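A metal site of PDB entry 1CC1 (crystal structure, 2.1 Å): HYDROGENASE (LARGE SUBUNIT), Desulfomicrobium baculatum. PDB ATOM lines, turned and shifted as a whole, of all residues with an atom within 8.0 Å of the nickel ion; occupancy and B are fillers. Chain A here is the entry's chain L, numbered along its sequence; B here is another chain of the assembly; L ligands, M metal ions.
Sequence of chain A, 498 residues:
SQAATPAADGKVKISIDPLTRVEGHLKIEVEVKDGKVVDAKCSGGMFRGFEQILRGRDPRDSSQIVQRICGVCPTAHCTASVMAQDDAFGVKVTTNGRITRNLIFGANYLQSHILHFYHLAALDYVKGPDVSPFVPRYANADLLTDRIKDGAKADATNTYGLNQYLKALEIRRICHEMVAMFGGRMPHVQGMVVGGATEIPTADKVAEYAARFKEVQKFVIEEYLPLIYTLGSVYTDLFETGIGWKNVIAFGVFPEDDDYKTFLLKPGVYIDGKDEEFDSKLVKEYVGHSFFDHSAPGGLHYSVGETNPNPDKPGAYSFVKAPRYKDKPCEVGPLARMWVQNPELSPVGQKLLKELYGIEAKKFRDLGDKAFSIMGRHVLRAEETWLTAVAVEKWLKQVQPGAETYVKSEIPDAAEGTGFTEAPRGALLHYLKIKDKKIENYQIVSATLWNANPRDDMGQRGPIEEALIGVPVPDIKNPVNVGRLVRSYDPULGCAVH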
ATOM      1  N   GLU A  23      20.059  -5.150  12.038  1.00  0.00           N
ATOM      2  CA  GLU A  23      20.827  -4.285  11.134  1.00  0.00           C
ATOM      3  C   GLU A  23      22.290  -4.467  11.502  1.00  0.00           C
ATOM      4  O   GLU A  23      22.640  -4.535  12.676  1.00  0.00           O
ATOM      5  CB  GLU A  23      20.415  -2.806  11.249  1.00  0.00           C
ATOM      6  CG  GLU A  23      21.074  -1.832  10.194  1.00  0.00           C
ATOM      7  CD  GLU A  23      22.610  -1.586  10.376  1.00  0.00           C
ATOM      8  OE1 GLU A  23      23.104  -1.464  11.519  1.00  0.00           O
ATOM      9  OE2 GLU A  23      23.316  -1.482   9.349  1.00  0.00           O
ATOM     10  N   GLN A  67      24.538  10.765   9.234  1.00  0.00           N
ATOM     11  CA  GLN A  67      23.369  10.030   8.741  1.00  0.00           C
ATOM     12  C   GLN A  67      23.799   8.686   8.166  1.00  0.00           C
ATOM     13  O   GLN A  67      23.072   7.698   8.287  1.00  0.00           O
ATOM     14  CB  GLN A  67      22.596  10.830   7.704  1.00  0.00           C
ATOM     15  CG  GLN A  67      21.692  11.878   8.319  1.00  0.00           C
ATOM     16  CD  GLN A  67      20.725  12.515   7.338  1.00  0.00           C
ATOM     17  OE1 GLN A  67      20.935  13.619   6.853  1.00  0.00           O
ATOM     18  NE2 GLN A  67      19.650  11.807   7.049  1.00  0.00           N
ATOM     19  N   ILE A  69      25.726   6.654   9.336  1.00  0.00           N
ATOM     20  CA  ILE A  69      26.008   5.687  10.407  1.00  0.00           C
ATOM     21  C   ILE A  69      24.960   4.577  10.232  1.00  0.00           C
ATOM     22  O   ILE A  69      25.253   3.387  10.398  1.00  0.00           O
ATOM     23  CB  ILE A  69      25.847   6.320  11.822  1.00  0.00           C
ATOM     24  CG1 ILE A  69      27.073   7.151  12.171  1.00  0.00           C
ATOM     25  CG2 ILE A  69      25.570   5.222  12.861  1.00  0.00           C
ATOM     26  CD1 ILE A  69      26.844   8.129  13.303  1.00  0.00           C
ATOM     27  N   CYS A  70      23.756   4.984   9.820  1.00  0.00           N
ATOM     28  CA  CYS A  70      22.690   4.027   9.618  1.00  0.00           C
ATOM     29  C   CYS A  70      21.616   4.453   8.635  1.00  0.00           C
ATOM     30  O   CYS A  70      20.970   5.477   8.844  1.00  0.00           O
ATOM     31  CB  CYS A  70      22.033   3.694  10.939  1.00  0.00           C
ATOM     32  SG  CYS A  70      20.794   2.397  10.725  1.00  0.00           S
ATOM     33  N   GLY A  71      21.391   3.635   7.613  1.00  0.00           N
ATOM     34  CA  GLY A  71      20.390   3.924   6.603  1.00  0.00           C
ATOM     35  C   GLY A  71      18.953   3.613   7.006  1.00  0.00           C
ATOM     36  O   GLY A  71      17.999   3.930   6.285  1.00  0.00           O
ATOM     37  N   VAL A  72      18.805   2.992   8.166  1.00  0.00           N
ATOM     38  CA  VAL A  72      17.489   2.655   8.702  1.00  0.00           C
ATOM     39  C   VAL A  72      16.988   3.826   9.589  1.00  0.00           C
ATOM     40  O   VAL A  72      15.859   4.284   9.457  1.00  0.00           O
ATOM     41  CB  VAL A  72      17.541   1.319   9.540  1.00  0.00           C
ATOM     42  CG1 VAL A  72      16.207   1.048  10.215  1.00  0.00           C
ATOM     43  CG2 VAL A  72      17.931   0.140   8.632  1.00  0.00           C
ATOM     44  N   CYS A  73      17.878   4.376  10.415  1.00  0.00           N
ATOM     45  CA  CYS A  73      17.538   5.485  11.304  1.00  0.00           C
ATOM     46  C   CYS A  73      18.409   6.737  11.075  1.00  0.00           C
ATOM     47  O   CYS A  73      18.848   7.373  12.045  1.00  0.00           O
ATOM     48  CB  CYS A  73      17.725   5.032  12.735  1.00  0.00           C
ATOM     49  SG  CYS A  73      19.471   4.785  13.171  1.00  0.00           S
ATOM     50  N   PRO A  74      18.557   7.174   9.818  1.00  0.00           N
ATOM     51  CA  PRO A  74      19.388   8.357   9.577  1.00  0.00           C
ATOM     52  C   PRO A  74      18.827   9.666  10.192  1.00  0.00           C
ATOM     53  O   PRO A  74      19.583  10.497  10.654  1.00  0.00           O
ATOM     54  CB  PRO A  74      19.484   8.415   8.051  1.00  0.00           C
ATOM     55  CG  PRO A  74      18.142   7.861   7.616  1.00  0.00           C
ATOM     56  CD  PRO A  74      17.948   6.693   8.557  1.00  0.00           C
ATOM     57  N   ALA A  76      17.304  10.075  12.952  1.00  0.00           N
ATOM     58  CA  ALA A  76      17.582  10.152  14.395  1.00  0.00           C
ATOM     59  C   ALA A  76      18.944  10.808  14.619  1.00  0.00           C
ATOM     60  O   ALA A  76      19.089  11.739  15.419  1.00  0.00           O
ATOM     61  CB  ALA A  76      17.546   8.777  15.025  1.00  0.00           C
ATOM     62  N   HIS A  77      19.936  10.353  13.849  1.00  0.00           N
ATOM     63  CA  HIS A  77      21.285  10.895  13.941  1.00  0.00           C
ATOM     64  C   HIS A  77      21.337  12.320  13.426  1.00  0.00           C
ATOM     65  O   HIS A  77      22.029  13.165  13.983  1.00  0.00           O
ATOM     66  CB  HIS A  77      22.285  10.035  13.171  1.00  0.00           C
ATOM     67  CG  HIS A  77      22.562   8.720  13.817  1.00  0.00           C
ATOM     68  ND1 HIS A  77      23.401   8.592  14.910  1.00  0.00           N
ATOM     69  CD2 HIS A  77      22.108   7.479  13.543  1.00  0.00           C
ATOM     70  CE1 HIS A  77      23.443   7.321  15.272  1.00  0.00           C
ATOM     71  NE2 HIS A  77      22.671   6.621  14.466  1.00  0.00           N
ATOM     72  N   ASN A 108       9.689   8.586   9.937  1.00  0.00           N
ATOM     73  CA  ASN A 108      10.610   7.481   9.950  1.00  0.00           C
ATOM     74  C   ASN A 108      10.498   6.601  11.190  1.00  0.00           C
ATOM     75  O   ASN A 108      10.943   5.446  11.173  1.00  0.00           O
ATOM     76  CB  ASN A 108      12.060   7.907   9.750  1.00  0.00           C
ATOM     77  CG  ASN A 108      12.926   6.751   9.271  1.00  0.00           C
ATOM     78  OD1 ASN A 108      12.653   6.189   8.213  1.00  0.00           O
ATOM     79  ND2 ASN A 108      13.905   6.344  10.076  1.00  0.00           N
ATOM     80  N   SER A 112      10.490   2.735  10.509  1.00  0.00           N
ATOM     81  CA  SER A 112      11.426   1.897  11.257  1.00  0.00           C
ATOM     82  C   SER A 112      10.777   0.759  12.048  1.00  0.00           C
ATOM     83  O   SER A 112      11.200  -0.408  11.968  1.00  0.00           O
ATOM     84  CB  SER A 112      12.300   2.766  12.163  1.00  0.00           C
ATOM     85  OG  SER A 112      13.334   2.004  12.757  1.00  0.00           O
ATOM     86  N   ALA A 423      16.253   7.636  19.246  1.00  0.00           N
ATOM     87  CA  ALA A 423      16.158   7.024  17.935  1.00  0.00           C
ATOM     88  C   ALA A 423      15.102   5.939  18.130  1.00  0.00           C
ATOM     89  O   ALA A 423      14.738   5.629  19.286  1.00  0.00           O
ATOM     90  CB  ALA A 423      17.492   6.408  17.544  1.00  0.00           C
ATOM     91  N   PRO A 424      14.505   5.439  17.034  1.00  0.00           N
ATOM     92  CA  PRO A 424      13.491   4.385  17.164  1.00  0.00           C
ATOM     93  C   PRO A 424      13.964   3.209  18.068  1.00  0.00           C
ATOM     94  O   PRO A 424      13.158   2.583  18.737  1.00  0.00           O
ATOM     95  CB  PRO A 424      13.275   3.944  15.716  1.00  0.00           C
ATOM     96  CG  PRO A 424      13.363   5.245  14.989  1.00  0.00           C
ATOM     97  CD  PRO A 424      14.579   5.922  15.644  1.00  0.00           C
ATOM     98  N   ARG A 425      15.271   2.937  18.104  1.00  0.00           N
ATOM     99  CA  ARG A 425      15.856   1.851  18.901  1.00  0.00           C
ATOM    100  C   ARG A 425      16.307   2.224  20.292  1.00  0.00           C
ATOM    101  O   ARG A 425      16.679   1.352  21.069  1.00  0.00           O
ATOM    102  CB  ARG A 425      17.007   1.206  18.128  1.00  0.00           C
ATOM    103  CG  ARG A 425      16.510   0.325  17.027  1.00  0.00           C
ATOM    104  CD  ARG A 425      17.404   0.288  15.813  1.00  0.00           C
ATOM    105  NE  ARG A 425      16.708  -0.429  14.768  1.00  0.00           N
ATOM    106  CZ  ARG A 425      15.976   0.160  13.815  1.00  0.00           C
ATOM    107  NH1 ARG A 425      15.879   1.478  13.773  1.00  0.00           N
ATOM    108  NH2 ARG A 425      15.189  -0.586  13.035  1.00  0.00           N
ATOM    109  N   SER A 446      24.858   6.111  20.980  1.00  0.00           N
ATOM    110  CA  SER A 446      23.696   5.688  20.205  1.00  0.00           C
ATOM    111  C   SER A 446      22.867   4.425  20.375  1.00  0.00           C
ATOM    112  O   SER A 446      23.267   3.354  19.905  1.00  0.00           O
ATOM    113  CB  SER A 446      24.112   5.714  18.735  1.00  0.00           C
ATOM    114  OG  SER A 446      24.924   4.568  18.498  1.00  0.00           O
ATOM    115  N   ALA A 447      21.603   4.627  20.750  1.00  0.00           N
ATOM    116  CA  ALA A 447      20.625   3.541  20.828  1.00  0.00           C
ATOM    117  C   ALA A 447      21.048   2.113  21.175  1.00  0.00           C
ATOM    118  O   ALA A 447      21.121   1.757  22.340  1.00  0.00           O
ATOM    119  CB  ALA A 447      19.860   3.511  19.506  1.00  0.00           C
ATOM    120  N   THR A 448      21.307   1.300  20.136  1.00  0.00           N
ATOM    121  CA  THR A 448      21.723  -0.100  20.293  1.00  0.00           C
ATOM    122  C   THR A 448      23.005  -0.235  21.112  1.00  0.00           C
ATOM    123  O   THR A 448      23.286  -1.283  21.680  1.00  0.00           O
ATOM    124  CB  THR A 448      21.869  -0.836  18.927  1.00  0.00           C
ATOM    125  OG1 THR A 448      20.604  -0.812  18.244  1.00  0.00           O
ATOM    126  CG2 THR A 448      22.277  -2.285  19.125  1.00  0.00           C
ATOM    127  N   ASP A 490      15.440  -5.114  18.442  1.00  0.00           N
ATOM    128  CA  ASP A 490      15.594  -4.384  17.180  1.00  0.00           C
ATOM    129  C   ASP A 490      17.017  -3.773  17.134  1.00  0.00           C
ATOM    130  O   ASP A 490      17.171  -2.576  16.923  1.00  0.00           O
ATOM    131  CB  ASP A 490      14.481  -3.321  17.124  1.00  0.00           C
ATOM    132  CG  ASP A 490      14.463  -2.514  15.848  1.00  0.00           C
ATOM    133  OD1 ASP A 490      13.760  -1.492  15.847  1.00  0.00           O
ATOM    134  OD2 ASP A 490      15.126  -2.874  14.837  1.00  0.00           O
ATOM    135  N   PRO A 491      18.063  -4.603  17.318  1.00  0.00           N
ATOM    136  CA  PRO A 491      19.446  -4.084  17.282  1.00  0.00           C
ATOM    137  C   PRO A 491      19.928  -3.548  15.929  1.00  0.00           C
ATOM    138  O   PRO A 491      19.618  -4.094  14.870  1.00  0.00           O
ATOM    139  CB  PRO A 491      20.308  -5.262  17.758  1.00  0.00           C
ATOM    140  CG  PRO A 491      19.411  -6.424  17.903  1.00  0.00           C
ATOM    141  CD  PRO A 491      18.032  -6.077  17.407  1.00  0.00           C
ATOM    142  N   SEC A 492      20.669  -2.455  16.015  1.00  0.00           N
ATOM    143  CA  SEC A 492      21.262  -1.793  14.854  1.00  0.00           C
ATOM    144  CB  SEC A 492      20.640  -0.406  14.672  1.00  0.00           C
ATOM    145 SE   SEC A 492      21.188   0.353  13.041  1.00  0.00          SE
ATOM    146  C   SEC A 492      22.753  -1.654  15.155  1.00  0.00           C
ATOM    147  O   SEC A 492      23.177  -0.735  15.834  1.00  0.00           O
ATOM    148  N   LEU A 493      23.521  -2.661  14.734  1.00  0.00           N
ATOM    149  CA  LEU A 493      24.960  -2.665  14.992  1.00  0.00           C
ATOM    150  C   LEU A 493      25.726  -1.550  14.274  1.00  0.00           C
ATOM    151  O   LEU A 493      26.792  -1.152  14.738  1.00  0.00           O
ATOM    152  CB  LEU A 493      25.549  -4.058  14.741  1.00  0.00           C
ATOM    153  CG  LEU A 493      25.359  -5.073  15.875  1.00  0.00           C
ATOM    154  CD1 LEU A 493      26.019  -4.556  17.143  1.00  0.00           C
ATOM    155  CD2 LEU A 493      23.873  -5.372  16.136  1.00  0.00           C
ATOM    156  N   GLY A 494      25.175  -1.024  13.181  1.00  0.00           N
ATOM    157  CA  GLY A 494      25.834   0.062  12.487  1.00  0.00           C
ATOM    158  C   GLY A 494      25.855   1.243  13.442  1.00  0.00           C
ATOM    159  O   GLY A 494      26.882   1.920  13.595  1.00  0.00           O
ATOM    160  N   CYS A 495      24.738   1.415  14.162  1.00  0.00           N
ATOM    161  CA  CYS A 495      24.590   2.473  15.156  1.00  0.00           C
ATOM    162  C   CYS A 495      25.388   2.217  16.415  1.00  0.00           C
ATOM    163  O   CYS A 495      26.037   3.100  16.925  1.00  0.00           O
ATOM    164  CB  CYS A 495      23.124   2.640  15.553  1.00  0.00           C
ATOM    165  SG  CYS A 495      22.147   3.557  14.343  1.00  0.00           S
ATOM    166  N   ALA A 496      25.329   0.992  16.923  1.00  0.00           N
ATOM    167  CA  ALA A 496      26.030   0.612  18.124  1.00  0.00           C
ATOM    168  C   ALA A 496      27.527   0.857  18.067  1.00  0.00           C
ATOM    169  O   ALA A 496      28.128   1.263  19.065  1.00  0.00           O
ATOM    170  CB  ALA A 496      25.752  -0.838  18.436  1.00  0.00           C
ATOM    171  N   CYS B  18      25.892   1.002   5.808  1.00  0.00           N
ATOM    172  CA  CYS B  18      24.945   1.493   6.793  1.00  0.00           C
ATOM    173  C   CYS B  18      23.555   0.875   6.587  1.00  0.00           C
ATOM    174  O   CYS B  18      22.624   1.172   7.358  1.00  0.00           O
ATOM    175  CB  CYS B  18      24.836   2.999   6.700  1.00  0.00           C
ATOM    176  SG  CYS B  18      23.774   3.593   5.347  1.00  0.00           S
ATOM    177  N   THR B  19      23.420   0.001   5.581  1.00  0.00           N
ATOM    178  CA  THR B  19      22.166  -0.694   5.221  1.00  0.00           C
ATOM    179  C   THR B  19      21.218   0.276   4.446  1.00  0.00           C
ATOM    180  O   THR B  19      20.119  -0.109   4.044  1.00  0.00           O
ATOM    181  CB  THR B  19      21.462  -1.356   6.463  1.00  0.00           C
ATOM    182  OG1 THR B  19      22.368  -2.298   7.056  1.00  0.00           O
ATOM    183  CG2 THR B  19      20.190  -2.103   6.071  1.00  0.00           C
HETATM  184 FE1  LIG L   1      19.912   3.715  15.138  1.00  0.00          FE
HETATM  185  C1  LIG L   1      20.260   2.454  16.481  1.00  0.00           C
HETATM  186  N1  LIG L   1      20.305   1.646  17.336  1.00  0.00           N
HETATM  187  C2  LIG L   1      18.060   3.564  15.411  1.00  0.00           C
HETATM  188  N2  LIG L   1      16.920   3.560  15.695  1.00  0.00           N
HETATM  189  C3  LIG L   1      20.344   5.235  16.184  1.00  0.00           C
HETATM  190  O1  LIG L   1      20.582   6.014  17.054  1.00  0.00           O
HETATM  191  S1  LG2 L   2      15.131   7.632  12.475  1.00  0.00           S
HETATM  192 NI    NI M   1      20.192   2.593  12.884  1.00  0.00          NI
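Within 4 Å of the nickel ion: Cys 70, Cys 73, SEC 492 and Cys 495. Along chain A the residues within 4 Å of the nickel ion span positions 70 to 495.
N of SEC 492 is in hydrogen-bond range of the side-chain hydroxyl of Thr 448. A ring nitrogen (NE2) of His 77 sits close to the side-chain sulfur (SG) of Cys 495 (3.1 Å). The side-chain sulfur of Cys 70 sits close to the backbone NH of Val 72. The backbone carbonyl oxygen (O) of Cys 495 is in hydrogen-bond range of the side-chain hydroxyl (OG) of Ser 446, 2.4 Å away.
The nickel ion is bound by SG of Cys 70 (2.2 Å), SG of Cys 73 (2.3 Å), SE of SEC 492 (2.5 Å) and SG of Cys 495 (2.6 Å).
N of Ala 76 lies close to S1 of LG2 L2. The side-chain sulfur (SG) of Cys 73 is bound to an iron atom (FE1) of LIG L1 (2.3 Å). The backbone NH (N) of Thr 448 is in hydrogen-bond range of a nitrogen (N1) of LIG L1 (3.0 Å). A nitrogen (N1) of LIG L1 lies within hydrogen-bond range of the side-chain hydroxyl (OG1) of Thr 448 (2.6 Å). NE2 of His 77 sits close to O1 of LIG L1 (3.4 Å). NH1 of Arg 425 sits at hydrogen-bond distance from N2 of LIG L1, at 3.0 Å. N of Arg 425 is in hydrogen-bond range of N2 of LIG L1 (3.0 Å). An iron atom (FE1) of LIG L1 is bound by the side-chain sulfur of Cys 495 (2.4 Å). S1 of LG2 L2 sits close to O of Cys 73, at 3.8 Å. ND2 of Asn 108 sits close to S1 of LG2 L2, 3.0 Å away.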
